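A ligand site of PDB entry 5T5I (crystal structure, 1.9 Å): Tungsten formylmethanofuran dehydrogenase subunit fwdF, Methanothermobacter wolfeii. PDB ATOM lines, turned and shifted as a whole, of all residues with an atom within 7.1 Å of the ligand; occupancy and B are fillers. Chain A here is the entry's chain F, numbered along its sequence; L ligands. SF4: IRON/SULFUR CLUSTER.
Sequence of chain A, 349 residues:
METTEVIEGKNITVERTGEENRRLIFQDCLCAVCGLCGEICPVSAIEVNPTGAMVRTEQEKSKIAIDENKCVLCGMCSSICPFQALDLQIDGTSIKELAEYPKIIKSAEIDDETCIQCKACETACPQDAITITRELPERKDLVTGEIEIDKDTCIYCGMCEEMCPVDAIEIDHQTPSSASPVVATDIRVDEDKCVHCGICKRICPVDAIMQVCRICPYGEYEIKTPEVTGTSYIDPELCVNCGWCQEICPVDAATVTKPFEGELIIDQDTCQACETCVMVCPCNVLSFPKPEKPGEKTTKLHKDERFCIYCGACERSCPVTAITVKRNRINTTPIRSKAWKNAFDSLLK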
ATOM      1  N   CYS A  34     -17.442  19.868  25.284  1.00  0.00           N
ATOM      2  CA  CYS A  34     -18.024  20.849  26.219  1.00  0.00           C
ATOM      3  C   CYS A  34     -17.091  22.038  26.483  1.00  0.00           C
ATOM      4  O   CYS A  34     -17.578  23.138  26.778  1.00  0.00           O
ATOM      5  CB  CYS A  34     -18.454  20.167  27.515  1.00  0.00           C
ATOM      6  SG  CYS A  34     -17.092  19.589  28.571  1.00  0.00           S
ATOM      7  N   PHE A  83     -17.585  13.413  30.981  1.00  0.00           N
ATOM      8  CA  PHE A  83     -17.814  12.380  29.974  1.00  0.00           C
ATOM      9  C   PHE A  83     -16.789  11.235  29.970  1.00  0.00           C
ATOM     10  O   PHE A  83     -16.821  10.404  29.068  1.00  0.00           O
ATOM     11  CB  PHE A  83     -17.863  13.083  28.595  1.00  0.00           C
ATOM     12  CG  PHE A  83     -18.977  14.116  28.531  1.00  0.00           C
ATOM     13  CD1 PHE A  83     -20.285  13.749  28.196  1.00  0.00           C
ATOM     14  CD2 PHE A  83     -18.742  15.442  28.871  1.00  0.00           C
ATOM     15  CE1 PHE A  83     -21.309  14.693  28.216  1.00  0.00           C
ATOM     16  CE2 PHE A  83     -19.765  16.389  28.850  1.00  0.00           C
ATOM     17  CZ  PHE A  83     -21.050  16.005  28.546  1.00  0.00           C
ATOM     18  N   CYS A 242     -27.430  12.006  33.515  1.00  0.00           N
ATOM     19  CA  CYS A 242     -28.486  12.936  33.096  1.00  0.00           C
ATOM     20  C   CYS A 242     -29.789  12.748  33.908  1.00  0.00           C
ATOM     21  O   CYS A 242     -30.501  13.719  34.081  1.00  0.00           O
ATOM     22  CB  CYS A 242     -28.736  12.814  31.603  1.00  0.00           C
ATOM     23  SG  CYS A 242     -29.510  11.257  31.117  1.00  0.00           S
ATOM     24  N   LEU A 264     -29.984  27.152  33.218  1.00  0.00           N
ATOM     25  CA  LEU A 264     -29.924  27.419  31.776  1.00  0.00           C
ATOM     26  C   LEU A 264     -30.787  28.629  31.514  1.00  0.00           C
ATOM     27  O   LEU A 264     -31.891  28.681  32.044  1.00  0.00           O
ATOM     28  CB  LEU A 264     -30.528  26.283  30.943  1.00  0.00           C
ATOM     29  CG  LEU A 264     -29.826  24.969  30.868  1.00  0.00           C
ATOM     30  CD1 LEU A 264     -30.602  24.023  29.937  1.00  0.00           C
ATOM     31  CD2 LEU A 264     -28.437  25.130  30.346  1.00  0.00           C
ATOM     32  N   CYS A 277     -27.544  23.450  19.010  1.00  0.00           N
ATOM     33  CA  CYS A 277     -27.527  23.061  20.427  1.00  0.00           C
ATOM     34  C   CYS A 277     -28.326  21.778  20.690  1.00  0.00           C
ATOM     35  O   CYS A 277     -27.900  20.936  21.479  1.00  0.00           O
ATOM     36  CB  CYS A 277     -28.020  24.213  21.308  1.00  0.00           C
ATOM     37  SG  CYS A 277     -29.760  24.697  21.016  1.00  0.00           S
ATOM     38  N   VAL A 280     -26.124  18.954  19.604  1.00  0.00           N
ATOM     39  CA  VAL A 280     -24.938  18.912  20.466  1.00  0.00           C
ATOM     40  C   VAL A 280     -25.212  18.331  21.847  1.00  0.00           C
ATOM     41  O   VAL A 280     -24.358  17.621  22.379  1.00  0.00           O
ATOM     42  CB  VAL A 280     -24.311  20.352  20.537  1.00  0.00           C
ATOM     43  CG1 VAL A 280     -23.480  20.584  21.799  1.00  0.00           C
ATOM     44  CG2 VAL A 280     -23.491  20.626  19.273  1.00  0.00           C
ATOM     45  N   CYS A 281     -26.362  18.676  22.451  1.00  0.00           N
ATOM     46  CA  CYS A 281     -26.631  18.282  23.833  1.00  0.00           C
ATOM     47  C   CYS A 281     -26.535  16.752  24.027  1.00  0.00           C
ATOM     48  O   CYS A 281     -27.310  16.024  23.419  1.00  0.00           O
ATOM     49  CB  CYS A 281     -27.965  18.807  24.323  1.00  0.00           C
ATOM     50  SG  CYS A 281     -28.388  18.281  26.010  1.00  0.00           S
ATOM     51  N   PRO A 282     -25.582  16.271  24.837  1.00  0.00           N
ATOM     52  CA  PRO A 282     -25.474  14.809  25.053  1.00  0.00           C
ATOM     53  C   PRO A 282     -26.515  14.241  26.012  1.00  0.00           C
ATOM     54  O   PRO A 282     -26.549  13.014  26.160  1.00  0.00           O
ATOM     55  CB  PRO A 282     -24.065  14.646  25.613  1.00  0.00           C
ATOM     56  CG  PRO A 282     -23.771  15.926  26.283  1.00  0.00           C
ATOM     57  CD  PRO A 282     -24.576  17.007  25.629  1.00  0.00           C
ATOM     58  N   CYS A 283     -27.348  15.081  26.655  1.00  0.00           N
ATOM     59  CA  CYS A 283     -28.369  14.637  27.605  1.00  0.00           C
ATOM     60  C   CYS A 283     -29.802  14.791  27.090  1.00  0.00           C
ATOM     61  O   CYS A 283     -30.738  14.570  27.859  1.00  0.00           O
ATOM     62  CB  CYS A 283     -28.177  15.390  28.908  1.00  0.00           C
ATOM     63  SG  CYS A 283     -26.548  15.149  29.654  1.00  0.00           S
ATOM     64  N   ASN A 284     -29.990  15.164  25.819  1.00  0.00           N
ATOM     65  CA  ASN A 284     -31.319  15.355  25.217  1.00  0.00           C
ATOM     66  C   ASN A 284     -32.226  16.271  26.060  1.00  0.00           C
ATOM     67  O   ASN A 284     -33.398  15.995  26.276  1.00  0.00           O
ATOM     68  CB  ASN A 284     -31.960  13.990  24.914  1.00  0.00           C
ATOM     69  CG  ASN A 284     -31.232  13.219  23.821  1.00  0.00           C
ATOM     70  OD1 ASN A 284     -30.205  13.648  23.273  1.00  0.00           O
ATOM     71  ND2 ASN A 284     -31.779  12.058  23.452  1.00  0.00           N
ATOM     72  N   VAL A 285     -31.666  17.394  26.514  1.00  0.00           N
ATOM     73  CA  VAL A 285     -32.366  18.414  27.306  1.00  0.00           C
ATOM     74  C   VAL A 285     -33.212  19.304  26.400  1.00  0.00           C
ATOM     75  O   VAL A 285     -34.247  19.777  26.816  1.00  0.00           O
ATOM     76  CB  VAL A 285     -31.337  19.308  28.061  1.00  0.00           C
ATOM     77  CG1 VAL A 285     -31.992  20.535  28.712  1.00  0.00           C
ATOM     78  CG2 VAL A 285     -30.541  18.520  29.098  1.00  0.00           C
ATOM     79  N   LEU A 286     -32.706  19.605  25.200  1.00  0.00           N
ATOM     80  CA  LEU A 286     -33.281  20.593  24.291  1.00  0.00           C
ATOM     81  C   LEU A 286     -34.078  20.009  23.138  1.00  0.00           C
ATOM     82  O   LEU A 286     -33.692  18.998  22.562  1.00  0.00           O
ATOM     83  CB  LEU A 286     -32.113  21.456  23.776  1.00  0.00           C
ATOM     84  CG  LEU A 286     -31.255  22.129  24.862  1.00  0.00           C
ATOM     85  CD1 LEU A 286     -29.959  22.657  24.293  1.00  0.00           C
ATOM     86  CD2 LEU A 286     -32.022  23.237  25.578  1.00  0.00           C
ATOM     87  N   LYS A 303     -36.588  23.509  26.855  1.00  0.00           N
ATOM     88  CA  LYS A 303     -35.643  22.843  27.735  1.00  0.00           C
ATOM     89  C   LYS A 303     -36.410  22.084  28.834  1.00  0.00           C
ATOM     90  O   LYS A 303     -37.531  22.452  29.187  1.00  0.00           O
ATOM     91  CB  LYS A 303     -34.683  23.854  28.408  1.00  0.00           C
ATOM     92  CG  LYS A 303     -35.369  24.814  29.408  1.00  0.00           C
ATOM     93  CD  LYS A 303     -34.431  25.785  30.131  1.00  0.00           C
ATOM     94  CE  LYS A 303     -35.190  26.432  31.293  1.00  0.00           C
ATOM     95  NZ  LYS A 303     -34.373  27.409  32.031  1.00  0.00           N
ATOM     96  N   ASP A 304     -35.770  21.054  29.404  1.00  0.00           N
ATOM     97  CA  ASP A 304     -36.221  20.369  30.620  1.00  0.00           C
ATOM     98  C   ASP A 304     -34.951  20.119  31.431  1.00  0.00           C
ATOM     99  O   ASP A 304     -34.222  19.150  31.174  1.00  0.00           O
ATOM    100  CB  ASP A 304     -37.052  19.100  30.368  1.00  0.00           C
ATOM    101  CG  ASP A 304     -37.707  18.571  31.644  1.00  0.00           C
ATOM    102  OD1 ASP A 304     -37.176  18.824  32.751  1.00  0.00           O
ATOM    103  OD2 ASP A 304     -38.737  17.898  31.541  1.00  0.00           O
ATOM    104  N   GLU A 305     -34.687  21.025  32.384  1.00  0.00           N
ATOM    105  CA  GLU A 305     -33.491  20.993  33.244  1.00  0.00           C
ATOM    106  C   GLU A 305     -33.400  19.795  34.185  1.00  0.00           C
ATOM    107  O   GLU A 305     -32.310  19.572  34.716  1.00  0.00           O
ATOM    108  CB  GLU A 305     -33.330  22.298  34.053  1.00  0.00           C
ATOM    109  CG  GLU A 305     -32.805  23.463  33.237  1.00  0.00           C
ATOM    110  CD  GLU A 305     -32.446  24.680  34.077  1.00  0.00           C
ATOM    111  OE1 GLU A 305     -31.684  24.522  35.061  1.00  0.00           O
ATOM    112  OE2 GLU A 305     -32.863  25.795  33.710  1.00  0.00           O
ATOM    113  N   PHE A 307     -32.953  16.970  33.152  1.00  0.00           N
ATOM    114  CA  PHE A 307     -31.956  16.139  32.470  1.00  0.00           C
ATOM    115  C   PHE A 307     -30.610  16.832  32.239  1.00  0.00           C
ATOM    116  O   PHE A 307     -29.706  16.201  31.698  1.00  0.00           O
ATOM    117  CB  PHE A 307     -32.528  15.620  31.127  1.00  0.00           C
ATOM    118  CG  PHE A 307     -33.934  15.092  31.257  1.00  0.00           C
ATOM    119  CD1 PHE A 307     -34.216  14.037  32.103  1.00  0.00           C
ATOM    120  CD2 PHE A 307     -34.983  15.678  30.564  1.00  0.00           C
ATOM    121  CE1 PHE A 307     -35.532  13.608  32.284  1.00  0.00           C
ATOM    122  CE2 PHE A 307     -36.288  15.224  30.719  1.00  0.00           C
ATOM    123  CZ  PHE A 307     -36.557  14.187  31.570  1.00  0.00           C
ATOM    124  N   CYS A 308     -30.451  18.093  32.656  1.00  0.00           N
ATOM    125  CA  CYS A 308     -29.256  18.891  32.388  1.00  0.00           C
ATOM    126  C   CYS A 308     -28.143  18.580  33.400  1.00  0.00           C
ATOM    127  O   CYS A 308     -28.419  18.366  34.579  1.00  0.00           O
ATOM    128  CB  CYS A 308     -29.609  20.383  32.376  1.00  0.00           C
ATOM    129  SG  CYS A 308     -28.248  21.475  31.871  1.00  0.00           S
ATOM    130  N   ILE A 309     -26.887  18.541  32.921  1.00  0.00           N
ATOM    131  CA  ILE A 309     -25.711  18.342  33.760  1.00  0.00           C
ATOM    132  C   ILE A 309     -24.823  19.605  33.792  1.00  0.00           C
ATOM    133  O   ILE A 309     -23.751  19.535  34.403  1.00  0.00           O
ATOM    134  CB  ILE A 309     -24.899  17.063  33.415  1.00  0.00           C
ATOM    135  CG1 ILE A 309     -24.253  17.137  31.997  1.00  0.00           C
ATOM    136  CG2 ILE A 309     -25.802  15.826  33.608  1.00  0.00           C
ATOM    137  CD1 ILE A 309     -23.339  16.010  31.620  1.00  0.00           C
ATOM    138  N   TYR A 310     -25.234  20.719  33.114  1.00  0.00           N
ATOM    139  CA  TYR A 310     -24.528  22.017  33.112  1.00  0.00           C
ATOM    140  C   TYR A 310     -23.113  21.905  32.589  1.00  0.00           C
ATOM    141  O   TYR A 310     -22.206  22.530  33.116  1.00  0.00           O
ATOM    142  CB  TYR A 310     -24.576  22.668  34.518  1.00  0.00           C
ATOM    143  CG  TYR A 310     -25.994  22.714  35.030  1.00  0.00           C
ATOM    144  CD1 TYR A 310     -26.922  23.608  34.506  1.00  0.00           C
ATOM    145  CD2 TYR A 310     -26.463  21.726  35.890  1.00  0.00           C
ATOM    146  CE1 TYR A 310     -28.280  23.501  34.790  1.00  0.00           C
ATOM    147  CE2 TYR A 310     -27.812  21.647  36.237  1.00  0.00           C
ATOM    148  CZ  TYR A 310     -28.717  22.557  35.698  1.00  0.00           C
ATOM    149  OH  TYR A 310     -30.044  22.457  36.030  1.00  0.00           O
ATOM    150  N   CYS A 311     -22.927  21.091  31.515  1.00  0.00           N
ATOM    151  CA  CYS A 311     -21.634  20.881  30.883  1.00  0.00           C
ATOM    152  C   CYS A 311     -21.184  22.118  30.092  1.00  0.00           C
ATOM    153  O   CYS A 311     -19.984  22.345  29.970  1.00  0.00           O
ATOM    154  CB  CYS A 311     -21.642  19.619  30.008  1.00  0.00           C
ATOM    155  SG  CYS A 311     -22.633  19.745  28.488  1.00  0.00           S
ATOM    156  N   GLY A 312     -22.137  22.879  29.554  1.00  0.00           N
ATOM    157  CA  GLY A 312     -21.849  24.081  28.767  1.00  0.00           C
ATOM    158  C   GLY A 312     -21.677  23.882  27.267  1.00  0.00           C
ATOM    159  O   GLY A 312     -21.435  24.857  26.556  1.00  0.00           O
ATOM    160  N   ALA A 313     -21.843  22.640  26.735  1.00  0.00           N
ATOM    161  CA  ALA A 313     -21.673  22.392  25.288  1.00  0.00           C
ATOM    162  C   ALA A 313     -22.642  23.198  24.420  1.00  0.00           C
ATOM    163  O   ALA A 313     -22.215  23.738  23.387  1.00  0.00           O
ATOM    164  CB  ALA A 313     -21.792  20.907  24.974  1.00  0.00           C
ATOM    165  N   CYS A 314     -23.918  23.323  24.838  1.00  0.00           N
ATOM    166  CA  CYS A 314     -24.945  24.074  24.096  1.00  0.00           C
ATOM    167  C   CYS A 314     -24.522  25.526  23.903  1.00  0.00           C
ATOM    168  O   CYS A 314     -24.480  26.028  22.770  1.00  0.00           O
ATOM    169  CB  CYS A 314     -26.301  23.965  24.784  1.00  0.00           C
ATOM    170  SG  CYS A 314     -26.297  24.425  26.548  1.00  0.00           S
ATOM    171  N   GLU A 315     -24.173  26.205  25.015  1.00  0.00           N
ATOM    172  CA  GLU A 315     -23.732  27.608  24.993  1.00  0.00           C
ATOM    173  C   GLU A 315     -22.516  27.783  24.078  1.00  0.00           C
ATOM    174  O   GLU A 315     -22.471  28.704  23.271  1.00  0.00           O
ATOM    175  CB  GLU A 315     -23.406  28.121  26.412  1.00  0.00           C
ATOM    176  CG  GLU A 315     -22.706  29.476  26.424  1.00  0.00           C
ATOM    177  CD  GLU A 315     -22.519  30.188  27.750  1.00  0.00           C
ATOM    178  OE1 GLU A 315     -22.129  31.376  27.718  1.00  0.00           O
ATOM    179  OE2 GLU A 315     -22.806  29.593  28.812  1.00  0.00           O
ATOM    180  N   ILE A 323     -28.189  30.984  24.205  1.00  0.00           N
ATOM    181  CA  ILE A 323     -28.348  30.090  25.343  1.00  0.00           C
ATOM    182  C   ILE A 323     -27.108  30.204  26.226  1.00  0.00           C
ATOM    183  O   ILE A 323     -25.997  30.138  25.713  1.00  0.00           O
ATOM    184  CB  ILE A 323     -28.711  28.611  24.923  1.00  0.00           C
ATOM    185  CG1 ILE A 323     -28.828  27.686  26.176  1.00  0.00           C
ATOM    186  CG2 ILE A 323     -27.742  28.027  23.914  1.00  0.00           C
ATOM    187  CD1 ILE A 323     -29.616  26.289  25.921  1.00  0.00           C
ATOM    188  N   VAL A 325     -25.248  29.110  30.198  1.00  0.00           N
ATOM    189  CA  VAL A 325     -25.199  28.156  31.300  1.00  0.00           C
ATOM    190  C   VAL A 325     -24.537  28.806  32.518  1.00  0.00           C
ATOM    191  O   VAL A 325     -23.414  29.305  32.405  1.00  0.00           O
ATOM    192  CB  VAL A 325     -24.431  26.884  30.858  1.00  0.00           C
ATOM    193  CG1 VAL A 325     -24.377  25.842  31.976  1.00  0.00           C
ATOM    194  CG2 VAL A 325     -25.051  26.287  29.598  1.00  0.00           C
ATOM    195  N   ARG A 327     -23.315  27.896  36.469  1.00  0.00           N
ATOM    196  CA  ARG A 327     -22.916  26.755  37.283  1.00  0.00           C
ATOM    197  C   ARG A 327     -22.711  27.282  38.705  1.00  0.00           C
ATOM    198  O   ARG A 327     -21.896  28.165  38.904  1.00  0.00           O
ATOM    199  CB  ARG A 327     -21.636  26.168  36.691  1.00  0.00           C
ATOM    200  CG  ARG A 327     -21.362  24.746  37.096  1.00  0.00           C
ATOM    201  CD  ARG A 327     -20.171  24.171  36.349  1.00  0.00           C
ATOM    202  NE  ARG A 327     -20.446  24.052  34.919  1.00  0.00           N
ATOM    203  CZ  ARG A 327     -19.915  24.784  33.941  1.00  0.00           C
ATOM    204  NH1 ARG A 327     -19.022  25.731  34.209  1.00  0.00           N
ATOM    205  NH2 ARG A 327     -20.266  24.566  32.674  1.00  0.00           N
HETATM  206 FE1  SF4 L   1     -27.353  21.043  29.782  1.00  0.00          FE
HETATM  207 FE2  SF4 L   1     -27.328  19.782  27.315  1.00  0.00          FE
HETATM  208 FE3  SF4 L   1     -24.822  20.341  28.606  1.00  0.00          FE
HETATM  209 FE4  SF4 L   1     -26.424  22.424  27.537  1.00  0.00          FE
HETATM  210  S1  SF4 L   1     -25.524  20.647  26.425  1.00  0.00           S
HETATM  211  S2  SF4 L   1     -25.426  22.269  29.570  1.00  0.00           S
HETATM  212  S3  SF4 L   1     -28.492  21.614  27.875  1.00  0.00           S
HETATM  213  S4  SF4 L   1     -26.516  19.018  29.281  1.00  0.00           S
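A sulfur (S1) of the ligand lies close to the backbone NH of Cys 314.
An iron atom (FE4) of the ligand is bound by the side-chain sulfur of Cys 314, at 2.2 Å.
SG of Cys 281 binds FE2 of the ligand.
N of Cys 311 lies close to S2 of the ligand (3.4 Å).
The side-chain sulfur (SG) of Cys 311 binds an iron atom (FE3) of the ligand, 2.3 Å away.
SG of Cys 308 binds FE1 of the ligand (2.3 Å).
The backbone NH (N) of Gly 312 sits close to a sulfur (S2) of the ligand (3.3 Å).
The backbone NH (N) of Ile 309 sits close to a sulfur (S4) of the ligand (3.7 Å).
The backbone NH of Val 285 lies close to the side-chain sulfur of Cys 281, at 3.4 Å.
The side-chain sulfur (SG) of Cys 281 sits close to the backbone NH (N) of Cys 283.
SG of Cys 281 sits close to N of Asn 284.
N of Ala 313 lies close to SG of Cys 311, at 3.5 Å.
The backbone carbonyl oxygen of Tyr 310 is in hydrogen-bond range of the guanidinium group of Arg 327 (2.8 Å).
The side-chain hydroxyl of Tyr 310 lies within hydrogen-bond range of the side-chain carboxylate of Glu 305, 2.8 Å away.
The backbone carbonyl oxygen (O) of Val 285 sits at hydrogen-bond distance from the backbone NH (N) of Asp 304 (3.3 Å).
N of Leu 264 lies within hydrogen-bond range of OE2 of Glu 305.
Merely in contact with the ligand: Tyr 310 (3.7 Å), Val 285 (3.7 Å), Leu 264 (3.8 Å), Pro 282 (3.8 Å) and Cys 283 (3.9 Å).
The nearest printed residue that does not touch the ligand is Leu 286 (4.01 Å).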
